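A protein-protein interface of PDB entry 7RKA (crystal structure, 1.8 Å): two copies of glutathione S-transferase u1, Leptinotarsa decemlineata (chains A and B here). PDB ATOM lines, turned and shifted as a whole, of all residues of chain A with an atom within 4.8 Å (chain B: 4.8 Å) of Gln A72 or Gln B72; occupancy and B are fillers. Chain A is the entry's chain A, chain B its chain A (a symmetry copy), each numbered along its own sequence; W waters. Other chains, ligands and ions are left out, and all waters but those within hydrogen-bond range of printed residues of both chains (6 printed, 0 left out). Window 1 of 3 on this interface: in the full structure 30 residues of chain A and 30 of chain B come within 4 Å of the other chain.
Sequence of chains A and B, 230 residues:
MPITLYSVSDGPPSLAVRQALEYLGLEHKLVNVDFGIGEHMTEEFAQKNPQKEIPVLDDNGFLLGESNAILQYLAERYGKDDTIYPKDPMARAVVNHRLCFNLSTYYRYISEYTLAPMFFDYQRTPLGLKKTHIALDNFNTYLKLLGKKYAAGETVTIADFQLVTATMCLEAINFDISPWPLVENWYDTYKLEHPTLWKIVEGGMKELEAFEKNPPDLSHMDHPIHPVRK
The side-chain amide oxygen (OE1) of Gln A72 is in hydrogen-bond range of the side-chain amide nitrogen (ND2) of Asn B96 (3.4 Å).
The side-chain amide oxygen (OE1) of Gln B72 sits at hydrogen-bond distance from the side-chain amide nitrogen (ND2) of Asn A96.
The side-chain hydroxyl (OH) of Tyr B85 sits at hydrogen-bond distance from the side-chain amide oxygen (OD1) of Asn B96 (2.6 Å).
The side-chain hydroxyl (OH) of Tyr A85 sits at hydrogen-bond distance from the side-chain amide oxygen (OD1) of Asn A96 (2.6 Å).
NE2 of Gln B72 lies within hydrogen-bond range of OD1 of Asn B96 (3.1 Å).
The side-chain amide oxygen of Gln A72 sits close to the backbone carbonyl oxygen of Asn A68.
NE2 of Gln A72 lies close to OH of Tyr A85.
The side-chain amide nitrogen (NE2) of Gln A72 is in hydrogen-bond range of the side-chain amide oxygen (OD1) of Asn A96 (3.1 Å).
Among the printed residues, pairs that only touch across the chains: Ala A69 with Asn B96 (3.9 Å), Gln A72 with Gln B72 (3.98 Å) and Asn A96 with Ala B69 (3.9 Å).
Of the printed residues of chain B, Ala A69 touches Asn B96.
Gln A72 touches just these residues of chain B: Gln B72 (3.98 Å) and Asn B96 (3.4 Å).
Of the printed residues of chain B, Asn A96 touches Ala B69 and Gln B72.
Printed residues of chain A within 4 Å of Ala B69: Asn A96 (3.9 Å).
Of chain A, only Gln A72 and Asn A96 come within 4 Å of Gln B72.
Printed residues of chain A within 4 Å of Asn B96: Ala A69 (3.9 Å) and Gln A72 (3.4 Å).
The nearest printed residue of chain B that does not touch Gln A72 is Tyr B85 (5.5 Å).
The nearest printed residue of chain A that does not touch Gln B72 is Tyr A85 (5.5 Å).
Of the 13 printed residues of chain B, 3 touch a printed residue of chain A.
Of the 13 printed residues of chain A, 3 touch a printed residue of chain B.
Hydrophobic or aromatic side chains of chain A within 4 Å of the printed part of chain B: Ala A69.
Along chain A the printed residues that touch a printed residue of chain B span positions 69 to 96.
Among the printed residues, 5 pairs touch across the chains.
Among the printed residues, no Asp or Glu carboxylate lies within 4 Å of a Lys or Arg side-chain nitrogen of the other chain.
Ala A69 touches Asn B96, and with the chains exchanged Asn A96 touches Ala B69.
Gln A72 touches its own counterpart, Gln B72.
Gln A72 touches Asn B96, and with the chains exchanged Asn A96 touches Gln B72.
Water W2 lies within hydrogen-bond range of OE2 of Glu A76, ND2 of Asn B96, OH of Tyr A85 and OH of Tyr B85.
Water W6 lies within hydrogen-bond range of the side-chain carboxylate of Glu B76 (2.8 Å), the side-chain amide nitrogen of Asn A96 (3.0 Å), the side-chain hydroxyl of Tyr B85 (3.0 Å) and the side-chain hydroxyl of Tyr A85 (3.3 Å).
Water W5 lies within hydrogen-bond range of the side-chain amide oxygen (OE1) of Gln A72 (2.9 Å), the side-chain amide nitrogen (NE2) of Gln B72 (3.1 Å) and the backbone carbonyl oxygen (O) of Asn B96 (3.4 Å).
Water W1 lies within hydrogen-bond range of the side-chain amide oxygen (OE1) of Gln B72, the side-chain amide nitrogen (NE2) of Gln A72 and the backbone carbonyl oxygen (O) of Asn A96.
Water W3 lies within hydrogen-bond range of the backbone carbonyl oxygen of Ala B69 (2.9 Å), the side-chain amide nitrogen of Asn A96 (2.9 Å) and the backbone NH of Tyr B73 (3.4 Å).
Water W4 lies within hydrogen-bond range of O of Ala A69 (2.9 Å), ND2 of Asn B96 (2.9 Å) and N of Tyr A73 (3.4 Å).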
ATOM      1  N   ASN A  68     -24.894   6.042  -4.201  1.00  0.00           N
ATOM      2  CA  ASN A  68     -25.376   7.406  -3.945  1.00  0.00           C
ATOM      3  C   ASN A  68     -24.537   8.441  -4.705  1.00  0.00           C
ATOM      4  O   ASN A  68     -25.075   9.389  -5.306  1.00  0.00           O
ATOM      5  CB  ASN A  68     -25.350   7.730  -2.445  1.00  0.00           C
ATOM      6  CG  ASN A  68     -26.561   7.215  -1.706  1.00  0.00           C
ATOM      7  OD1 ASN A  68     -27.455   6.584  -2.283  1.00  0.00           O
ATOM      8  ND2 ASN A  68     -26.589   7.463  -0.402  1.00  0.00           N
ATOM      9  N   ALA A  69     -23.200   8.313  -4.621  1.00  0.00           N
ATOM     10  CA  ALA A  69     -22.303   9.263  -5.280  1.00  0.00           C
ATOM     11  C   ALA A  69     -22.406   9.159  -6.802  1.00  0.00           C
ATOM     12  O   ALA A  69     -22.329  10.178  -7.508  1.00  0.00           O
ATOM     13  CB  ALA A  69     -20.850   9.026  -4.844  1.00  0.00           C
ATOM     14  N   ILE A  70     -22.569   7.937  -7.323  1.00  0.00           N
ATOM     15  CA  ILE A  70     -22.807   7.773  -8.758  1.00  0.00           C
ATOM     16  C   ILE A  70     -24.061   8.533  -9.182  1.00  0.00           C
ATOM     17  O   ILE A  70     -24.067   9.239 -10.197  1.00  0.00           O
ATOM     18  CB  ILE A  70     -22.905   6.285  -9.124  1.00  0.00           C
ATOM     19  CG1 ILE A  70     -21.582   5.574  -8.853  1.00  0.00           C
ATOM     20  CG2 ILE A  70     -23.305   6.140 -10.584  1.00  0.00           C
ATOM     21  CD1 ILE A  70     -21.720   4.043  -8.770  1.00  0.00           C
ATOM     22  N   LEU A  71     -25.152   8.400  -8.416  1.00  0.00           N
ATOM     23  CA  LEU A  71     -26.396   9.085  -8.775  1.00  0.00           C
ATOM     24  C   LEU A  71     -26.257  10.606  -8.706  1.00  0.00           C
ATOM     25  O   LEU A  71     -26.739  11.345  -9.594  1.00  0.00           O
ATOM     26  CB  LEU A  71     -27.523   8.612  -7.845  1.00  0.00           C
ATOM     27  CG  LEU A  71     -28.044   7.202  -8.078  1.00  0.00           C
ATOM     28  CD1 LEU A  71     -28.913   6.801  -6.886  1.00  0.00           C
ATOM     29  CD2 LEU A  71     -28.793   7.130  -9.393  1.00  0.00           C
ATOM     30  N   GLN A  72     -25.605  11.097  -7.655  1.00  0.00           N
ATOM     31  CA  GLN A  72     -25.378  12.523  -7.513  1.00  0.00           C
ATOM     32  C   GLN A  72     -24.538  13.073  -8.661  1.00  0.00           C
ATOM     33  O   GLN A  72     -24.784  14.188  -9.128  1.00  0.00           O
ATOM     34  CB  GLN A  72     -24.703  12.814  -6.165  1.00  0.00           C
ATOM     35  CG  GLN A  72     -25.619  12.548  -4.970  1.00  0.00           C
ATOM     36  CD  GLN A  72     -24.884  12.406  -3.639  1.00  0.00           C
ATOM     37  OE1 GLN A  72     -23.771  11.875  -3.569  1.00  0.00           O
ATOM     38  NE2 GLN A  72     -25.560  12.805  -2.558  1.00  0.00           N
ATOM     39  N   TYR A  73     -23.556  12.302  -9.119  1.00  0.00           N
ATOM     40  CA  TYR A  73     -22.700  12.700 -10.238  1.00  0.00           C
ATOM     41  C   TYR A  73     -23.468  12.692 -11.554  1.00  0.00           C
ATOM     42  O   TYR A  73     -23.435  13.676 -12.315  1.00  0.00           O
ATOM     43  CB  TYR A  73     -21.498  11.745 -10.321  1.00  0.00           C
ATOM     44  CG  TYR A  73     -20.723  11.860 -11.618  1.00  0.00           C
ATOM     45  CD1 TYR A  73     -19.828  12.896 -11.806  1.00  0.00           C
ATOM     46  CD2 TYR A  73     -20.893  10.939 -12.652  1.00  0.00           C
ATOM     47  CE1 TYR A  73     -19.123  13.037 -12.995  1.00  0.00           C
ATOM     48  CE2 TYR A  73     -20.172  11.067 -13.860  1.00  0.00           C
ATOM     49  CZ  TYR A  73     -19.299  12.124 -14.014  1.00  0.00           C
ATOM     50  OH  TYR A  73     -18.588  12.293 -15.194  1.00  0.00           O
ATOM     51  N   LEU A  74     -24.164  11.589 -11.842  1.00  0.00           N
ATOM     52  CA  LEU A  74     -24.888  11.499 -13.109  1.00  0.00           C
ATOM     53  C   LEU A  74     -25.909  12.613 -13.237  1.00  0.00           C
ATOM     54  O   LEU A  74     -26.053  13.219 -14.308  1.00  0.00           O
ATOM     55  CB  LEU A  74     -25.587  10.144 -13.238  1.00  0.00           C
ATOM     56  CG  LEU A  74     -24.741   8.891 -13.458  1.00  0.00           C
ATOM     57  CD1 LEU A  74     -25.652   7.656 -13.363  1.00  0.00           C
ATOM     58  CD2 LEU A  74     -24.027   8.948 -14.804  1.00  0.00           C
ATOM     59  N   ALA A  75     -26.667  12.873 -12.160  1.00  0.00           N
ATOM     60  CA  ALA A  75     -27.711  13.882 -12.232  1.00  0.00           C
ATOM     61  C   ALA A  75     -27.149  15.301 -12.328  1.00  0.00           C
ATOM     62  O   ALA A  75     -27.760  16.157 -12.984  1.00  0.00           O
ATOM     63  CB  ALA A  75     -28.653  13.755 -11.031  1.00  0.00           C
ATOM     64  N   GLU A  76     -26.004  15.583 -11.699  1.00  0.00           N
ATOM     65  CA  GLU A  76     -25.445  16.928 -11.856  1.00  0.00           C
ATOM     66  C   GLU A  76     -24.798  17.125 -13.226  1.00  0.00           C
ATOM     67  O   GLU A  76     -24.865  18.220 -13.789  1.00  0.00           O
ATOM     68  CB  GLU A  76     -24.401  17.240 -10.780  1.00  0.00           C
ATOM     69  CG  GLU A  76     -24.914  17.143  -9.361  1.00  0.00           C
ATOM     70  CD  GLU A  76     -23.840  17.473  -8.338  1.00  0.00           C
ATOM     71  OE1 GLU A  76     -23.627  18.701  -8.134  1.00  0.00           O
ATOM     72  OE2 GLU A  76     -23.206  16.525  -7.788  1.00  0.00           O
ATOM     73  N   TYR A  85     -32.432  16.214  -9.289  1.00  0.00           N
ATOM     74  CA  TYR A  85     -31.436  16.565  -8.276  1.00  0.00           C
ATOM     75  C   TYR A  85     -31.308  18.087  -8.230  1.00  0.00           C
ATOM     76  O   TYR A  85     -30.350  18.664  -8.773  1.00  0.00           O
ATOM     77  CB  TYR A  85     -30.114  15.878  -8.588  1.00  0.00           C
ATOM     78  CG  TYR A  85     -29.144  15.838  -7.421  1.00  0.00           C
ATOM     79  CD1 TYR A  85     -29.580  15.581  -6.112  1.00  0.00           C
ATOM     80  CD2 TYR A  85     -27.797  16.056  -7.626  1.00  0.00           C
ATOM     81  CE1 TYR A  85     -28.670  15.549  -5.032  1.00  0.00           C
ATOM     82  CE2 TYR A  85     -26.889  15.999  -6.564  1.00  0.00           C
ATOM     83  CZ  TYR A  85     -27.340  15.749  -5.274  1.00  0.00           C
ATOM     84  OH  TYR A  85     -26.415  15.713  -4.244  1.00  0.00           O
ATOM     85  N   ASN A  96     -30.557  14.890  -0.530  1.00  0.00           N
ATOM     86  CA  ASN A  96     -29.353  14.332   0.094  1.00  0.00           C
ATOM     87  C   ASN A  96     -29.699  13.636   1.400  1.00  0.00           C
ATOM     88  O   ASN A  96     -29.118  12.588   1.738  1.00  0.00           O
ATOM     89  CB  ASN A  96     -28.309  15.434   0.340  1.00  0.00           C
ATOM     90  CG  ASN A  96     -27.566  15.862  -0.930  1.00  0.00           C
ATOM     91  OD1 ASN A  96     -27.549  15.163  -1.952  1.00  0.00           O
ATOM     92  ND2 ASN A  96     -26.952  17.024  -0.868  1.00  0.00           N
ATOM     93  N   LEU A  99     -31.198  10.248   0.572  1.00  0.00           N
ATOM     94  CA  LEU A  99     -30.144   9.326   0.148  1.00  0.00           C
ATOM     95  C   LEU A  99     -29.357   8.793   1.344  1.00  0.00           C
ATOM     96  O   LEU A  99     -29.025   7.594   1.405  1.00  0.00           O
ATOM     97  CB  LEU A  99     -29.216  10.032  -0.850  1.00  0.00           C
ATOM     98  CG  LEU A  99     -29.768  10.325  -2.243  1.00  0.00           C
ATOM     99  CD1 LEU A  99     -28.846  11.284  -2.972  1.00  0.00           C
ATOM    100  CD2 LEU A  99     -29.965   9.037  -3.044  1.00  0.00           C
ATOM    101  N   ILE A 158     -33.473  11.423  -7.562  1.00  0.00           N
ATOM    102  CA  ILE A 158     -32.592  10.276  -7.404  1.00  0.00           C
ATOM    103  C   ILE A 158     -32.800   9.568  -6.072  1.00  0.00           C
ATOM    104  O   ILE A 158     -32.467   8.388  -5.952  1.00  0.00           O
ATOM    105  CB  ILE A 158     -31.108  10.661  -7.572  1.00  0.00           C
ATOM    106  CG1 ILE A 158     -30.659  11.789  -6.622  1.00  0.00           C
ATOM    107  CG2 ILE A 158     -30.770  10.985  -9.014  1.00  0.00           C
ATOM    108  CD1 ILE A 158     -29.144  12.058  -6.736  1.00  0.00           C
ATOM    109  N   ASN B  68     -23.958  13.851   6.956  1.00  0.00           N
ATOM    110  CA  ASN B  68     -23.446  14.062   5.596  1.00  0.00           C
ATOM    111  C   ASN B  68     -24.245  15.149   4.866  1.00  0.00           C
ATOM    112  O   ASN B  68     -23.673  16.024   4.189  1.00  0.00           O
ATOM    113  CB  ASN B  68     -23.491  12.763   4.779  1.00  0.00           C
ATOM    114  CG  ASN B  68     -22.307  11.862   5.033  1.00  0.00           C
ATOM    115  OD1 ASN B  68     -21.419  12.168   5.840  1.00  0.00           O
ATOM    116  ND2 ASN B  68     -22.296  10.720   4.357  1.00  0.00           N
ATOM    117  N   ALA B  69     -25.587  15.061   4.934  1.00  0.00           N
ATOM    118  CA  ALA B  69     -26.447  16.026   4.250  1.00  0.00           C
ATOM    119  C   ALA B  69     -26.320  17.419   4.868  1.00  0.00           C
ATOM    120  O   ALA B  69     -26.359  18.432   4.149  1.00  0.00           O
ATOM    121  CB  ALA B  69     -27.913  15.573   4.298  1.00  0.00           C
ATOM    122  N   ILE B  70     -26.179  17.489   6.197  1.00  0.00           N
ATOM    123  CA  ILE B  70     -25.919  18.776   6.844  1.00  0.00           C
ATOM    124  C   ILE B  70     -24.639  19.401   6.296  1.00  0.00           C
ATOM    125  O   ILE B  70     -24.598  20.596   5.978  1.00  0.00           O
ATOM    126  CB  ILE B  70     -25.853  18.612   8.369  1.00  0.00           C
ATOM    127  CG1 ILE B  70     -27.198  18.149   8.922  1.00  0.00           C
ATOM    128  CG2 ILE B  70     -25.430  19.925   9.010  1.00  0.00           C
ATOM    129  CD1 ILE B  70     -27.101  17.547  10.335  1.00  0.00           C
ATOM    130  N   LEU B  71     -23.566  18.609   6.180  1.00  0.00           N
ATOM    131  CA  LEU B  71     -22.299  19.148   5.681  1.00  0.00           C
ATOM    132  C   LEU B  71     -22.400  19.604   4.225  1.00  0.00           C
ATOM    133  O   LEU B  71     -21.884  20.677   3.841  1.00  0.00           O
ATOM    134  CB  LEU B  71     -21.201  18.084   5.828  1.00  0.00           C
ATOM    135  CG  LEU B  71     -20.711  17.810   7.242  1.00  0.00           C
ATOM    136  CD1 LEU B  71     -19.874  16.532   7.229  1.00  0.00           C
ATOM    137  CD2 LEU B  71     -19.941  19.003   7.771  1.00  0.00           C
ATOM    138  N   GLN B  72     -23.059  18.799   3.394  1.00  0.00           N
ATOM    139  CA  GLN B  72     -23.251  19.157   2.001  1.00  0.00           C
ATOM    140  C   GLN B  72     -24.057  20.444   1.860  1.00  0.00           C
ATOM    141  O   GLN B  72     -23.775  21.256   0.975  1.00  0.00           O
ATOM    142  CB  GLN B  72     -23.943  18.005   1.256  1.00  0.00           C
ATOM    143  CG  GLN B  72     -23.055  16.768   1.115  1.00  0.00           C
ATOM    144  CD  GLN B  72     -23.817  15.488   0.783  1.00  0.00           C
ATOM    145  OE1 GLN B  72     -24.945  15.270   1.238  1.00  0.00           O
ATOM    146  NE2 GLN B  72     -23.150  14.590   0.051  1.00  0.00           N
ATOM    147  N   TYR B  73     -25.050  20.637   2.723  1.00  0.00           N
ATOM    148  CA  TYR B  73     -25.876  21.846   2.714  1.00  0.00           C
ATOM    149  C   TYR B  73     -25.085  23.061   3.184  1.00  0.00           C
ATOM    150  O   TYR B  73     -25.079  24.112   2.518  1.00  0.00           O
ATOM    151  CB  TYR B  73     -27.099  21.629   3.619  1.00  0.00           C
ATOM    152  CG  TYR B  73     -27.849  22.907   3.939  1.00  0.00           C
ATOM    153  CD1 TYR B  73     -28.714  23.459   3.013  1.00  0.00           C
ATOM    154  CD2 TYR B  73     -27.684  23.562   5.160  1.00  0.00           C
ATOM    155  CE1 TYR B  73     -29.393  24.643   3.273  1.00  0.00           C
ATOM    156  CE2 TYR B  73     -28.379  24.760   5.439  1.00  0.00           C
ATOM    157  CZ  TYR B  73     -29.222  25.286   4.482  1.00  0.00           C
ATOM    158  OH  TYR B  73     -29.908  26.471   4.712  1.00  0.00           O
ATOM    159  N   LEU B  74     -24.412  22.939   4.331  1.00  0.00           N
ATOM    160  CA  LEU B  74     -23.668  24.081   4.861  1.00  0.00           C
ATOM    161  C   LEU B  74     -22.617  24.554   3.874  1.00  0.00           C
ATOM    162  O   LEU B  74     -22.439  25.764   3.672  1.00  0.00           O
ATOM    163  CB  LEU B  74     -23.001  23.723   6.190  1.00  0.00           C
ATOM    164  CG  LEU B  74     -23.875  23.526   7.429  1.00  0.00           C
ATOM    165  CD1 LEU B  74     -22.997  22.993   8.573  1.00  0.00           C
ATOM    166  CD2 LEU B  74     -24.564  24.829   7.820  1.00  0.00           C
ATOM    167  N   ALA B  75     -21.872  23.611   3.277  1.00  0.00           N
ATOM    168  CA  ALA B  75     -20.802  23.996   2.371  1.00  0.00           C
ATOM    169  C   ALA B  75     -21.326  24.583   1.061  1.00  0.00           C
ATOM    170  O   ALA B  75     -20.682  25.475   0.490  1.00  0.00           O
ATOM    171  CB  ALA B  75     -19.885  22.800   2.098  1.00  0.00           C
ATOM    172  N   GLU B  76     -22.474  24.116   0.561  1.00  0.00           N
ATOM    173  CA  GLU B  76     -22.996  24.735  -0.660  1.00  0.00           C
ATOM    174  C   GLU B  76     -23.613  26.107  -0.390  1.00  0.00           C
ATOM    175  O   GLU B  76     -23.509  27.007  -1.227  1.00  0.00           O
ATOM    176  CB  GLU B  76     -24.051  23.856  -1.339  1.00  0.00           C
ATOM    177  CG  GLU B  76     -23.566  22.477  -1.722  1.00  0.00           C
ATOM    178  CD  GLU B  76     -24.649  21.654  -2.399  1.00  0.00           C
ATOM    179  OE1 GLU B  76     -24.835  21.885  -3.627  1.00  0.00           O
ATOM    180  OE2 GLU B  76     -25.316  20.831  -1.706  1.00  0.00           O
ATOM    181  N   TYR B  85     -16.076  21.903  -0.739  1.00  0.00           N
ATOM    182  CA  TYR B  85     -17.080  21.095  -1.432  1.00  0.00           C
ATOM    183  C   TYR B  85     -17.172  21.572  -2.881  1.00  0.00           C
ATOM    184  O   TYR B  85     -18.105  22.303  -3.255  1.00  0.00           O
ATOM    185  CB  TYR B  85     -18.414  21.188  -0.703  1.00  0.00           C
ATOM    186  CG  TYR B  85     -19.405  20.102  -1.080  1.00  0.00           C
ATOM    187  CD1 TYR B  85     -19.000  18.774  -1.277  1.00  0.00           C
ATOM    188  CD2 TYR B  85     -20.742  20.403  -1.239  1.00  0.00           C
ATOM    189  CE1 TYR B  85     -19.928  17.770  -1.631  1.00  0.00           C
ATOM    190  CE2 TYR B  85     -21.670  19.408  -1.564  1.00  0.00           C
ATOM    191  CZ  TYR B  85     -21.249  18.099  -1.759  1.00  0.00           C
ATOM    192  OH  TYR B  85     -22.193  17.142  -2.094  1.00  0.00           O
ATOM    193  N   ASN B  96     -18.140  13.266  -2.511  1.00  0.00           N
ATOM    194  CA  ASN B  96     -19.368  12.520  -2.221  1.00  0.00           C
ATOM    195  C   ASN B  96     -19.063  11.047  -2.005  1.00  0.00           C
ATOM    196  O   ASN B  96     -19.677  10.387  -1.145  1.00  0.00           O
ATOM    197  CB  ASN B  96     -20.388  12.690  -3.359  1.00  0.00           C
ATOM    198  CG  ASN B  96     -21.097  14.048  -3.342  1.00  0.00           C
ATOM    199  OD1 ASN B  96     -21.113  14.772  -2.337  1.00  0.00           O
ATOM    200  ND2 ASN B  96     -21.683  14.401  -4.466  1.00  0.00           N
ATOM    201  N   LEU B  99     -17.636  10.635   1.489  1.00  0.00           N
ATOM    202  CA  LEU B  99     -18.705  10.747   2.482  1.00  0.00           C
ATOM    203  C   LEU B  99     -19.526   9.461   2.561  1.00  0.00           C
ATOM    204  O   LEU B  99     -19.889   9.004   3.661  1.00  0.00           O
ATOM    205  CB  LEU B  99     -19.597  11.948   2.141  1.00  0.00           C
ATOM    206  CG  LEU B  99     -19.013  13.344   2.349  1.00  0.00           C
ATOM    207  CD1 LEU B  99     -19.898  14.379   1.680  1.00  0.00           C
ATOM    208  CD2 LEU B  99     -18.834  13.654   3.837  1.00  0.00           C
ATOM    209  N   ILE B 158     -15.188  18.623   3.195  1.00  0.00           N
ATOM    210  CA  ILE B 158     -16.100  18.107   4.204  1.00  0.00           C
ATOM    211  C   ILE B 158     -15.933  16.609   4.419  1.00  0.00           C
ATOM    212  O   ILE B 158     -16.299  16.104   5.482  1.00  0.00           O
ATOM    213  CB  ILE B 158     -17.570  18.434   3.872  1.00  0.00           C
ATOM    214  CG1 ILE B 158     -18.008  17.935   2.481  1.00  0.00           C
ATOM    215  CG2 ILE B 158     -17.875  19.908   4.053  1.00  0.00           C
ATOM    216  CD1 ILE B 158     -19.513  18.173   2.240  1.00  0.00           C
HETATM  217  O   HOH W   1     -26.001  12.716   0.514  1.00  0.00           O
HETATM  218  O   HOH W   2     -23.623  16.615  -4.973  1.00  0.00           O
HETATM  219  O   HOH W   3     -27.433  18.566   1.498  1.00  0.00           O
HETATM  220  O   HOH W   4     -21.205  12.689  -6.712  1.00  0.00           O
HETATM  221  O   HOH W   5     -22.767  11.661  -0.903  1.00  0.00           O
HETATM  222  O   HOH W   6     -24.947  18.205  -2.743  1.00  0.00           O
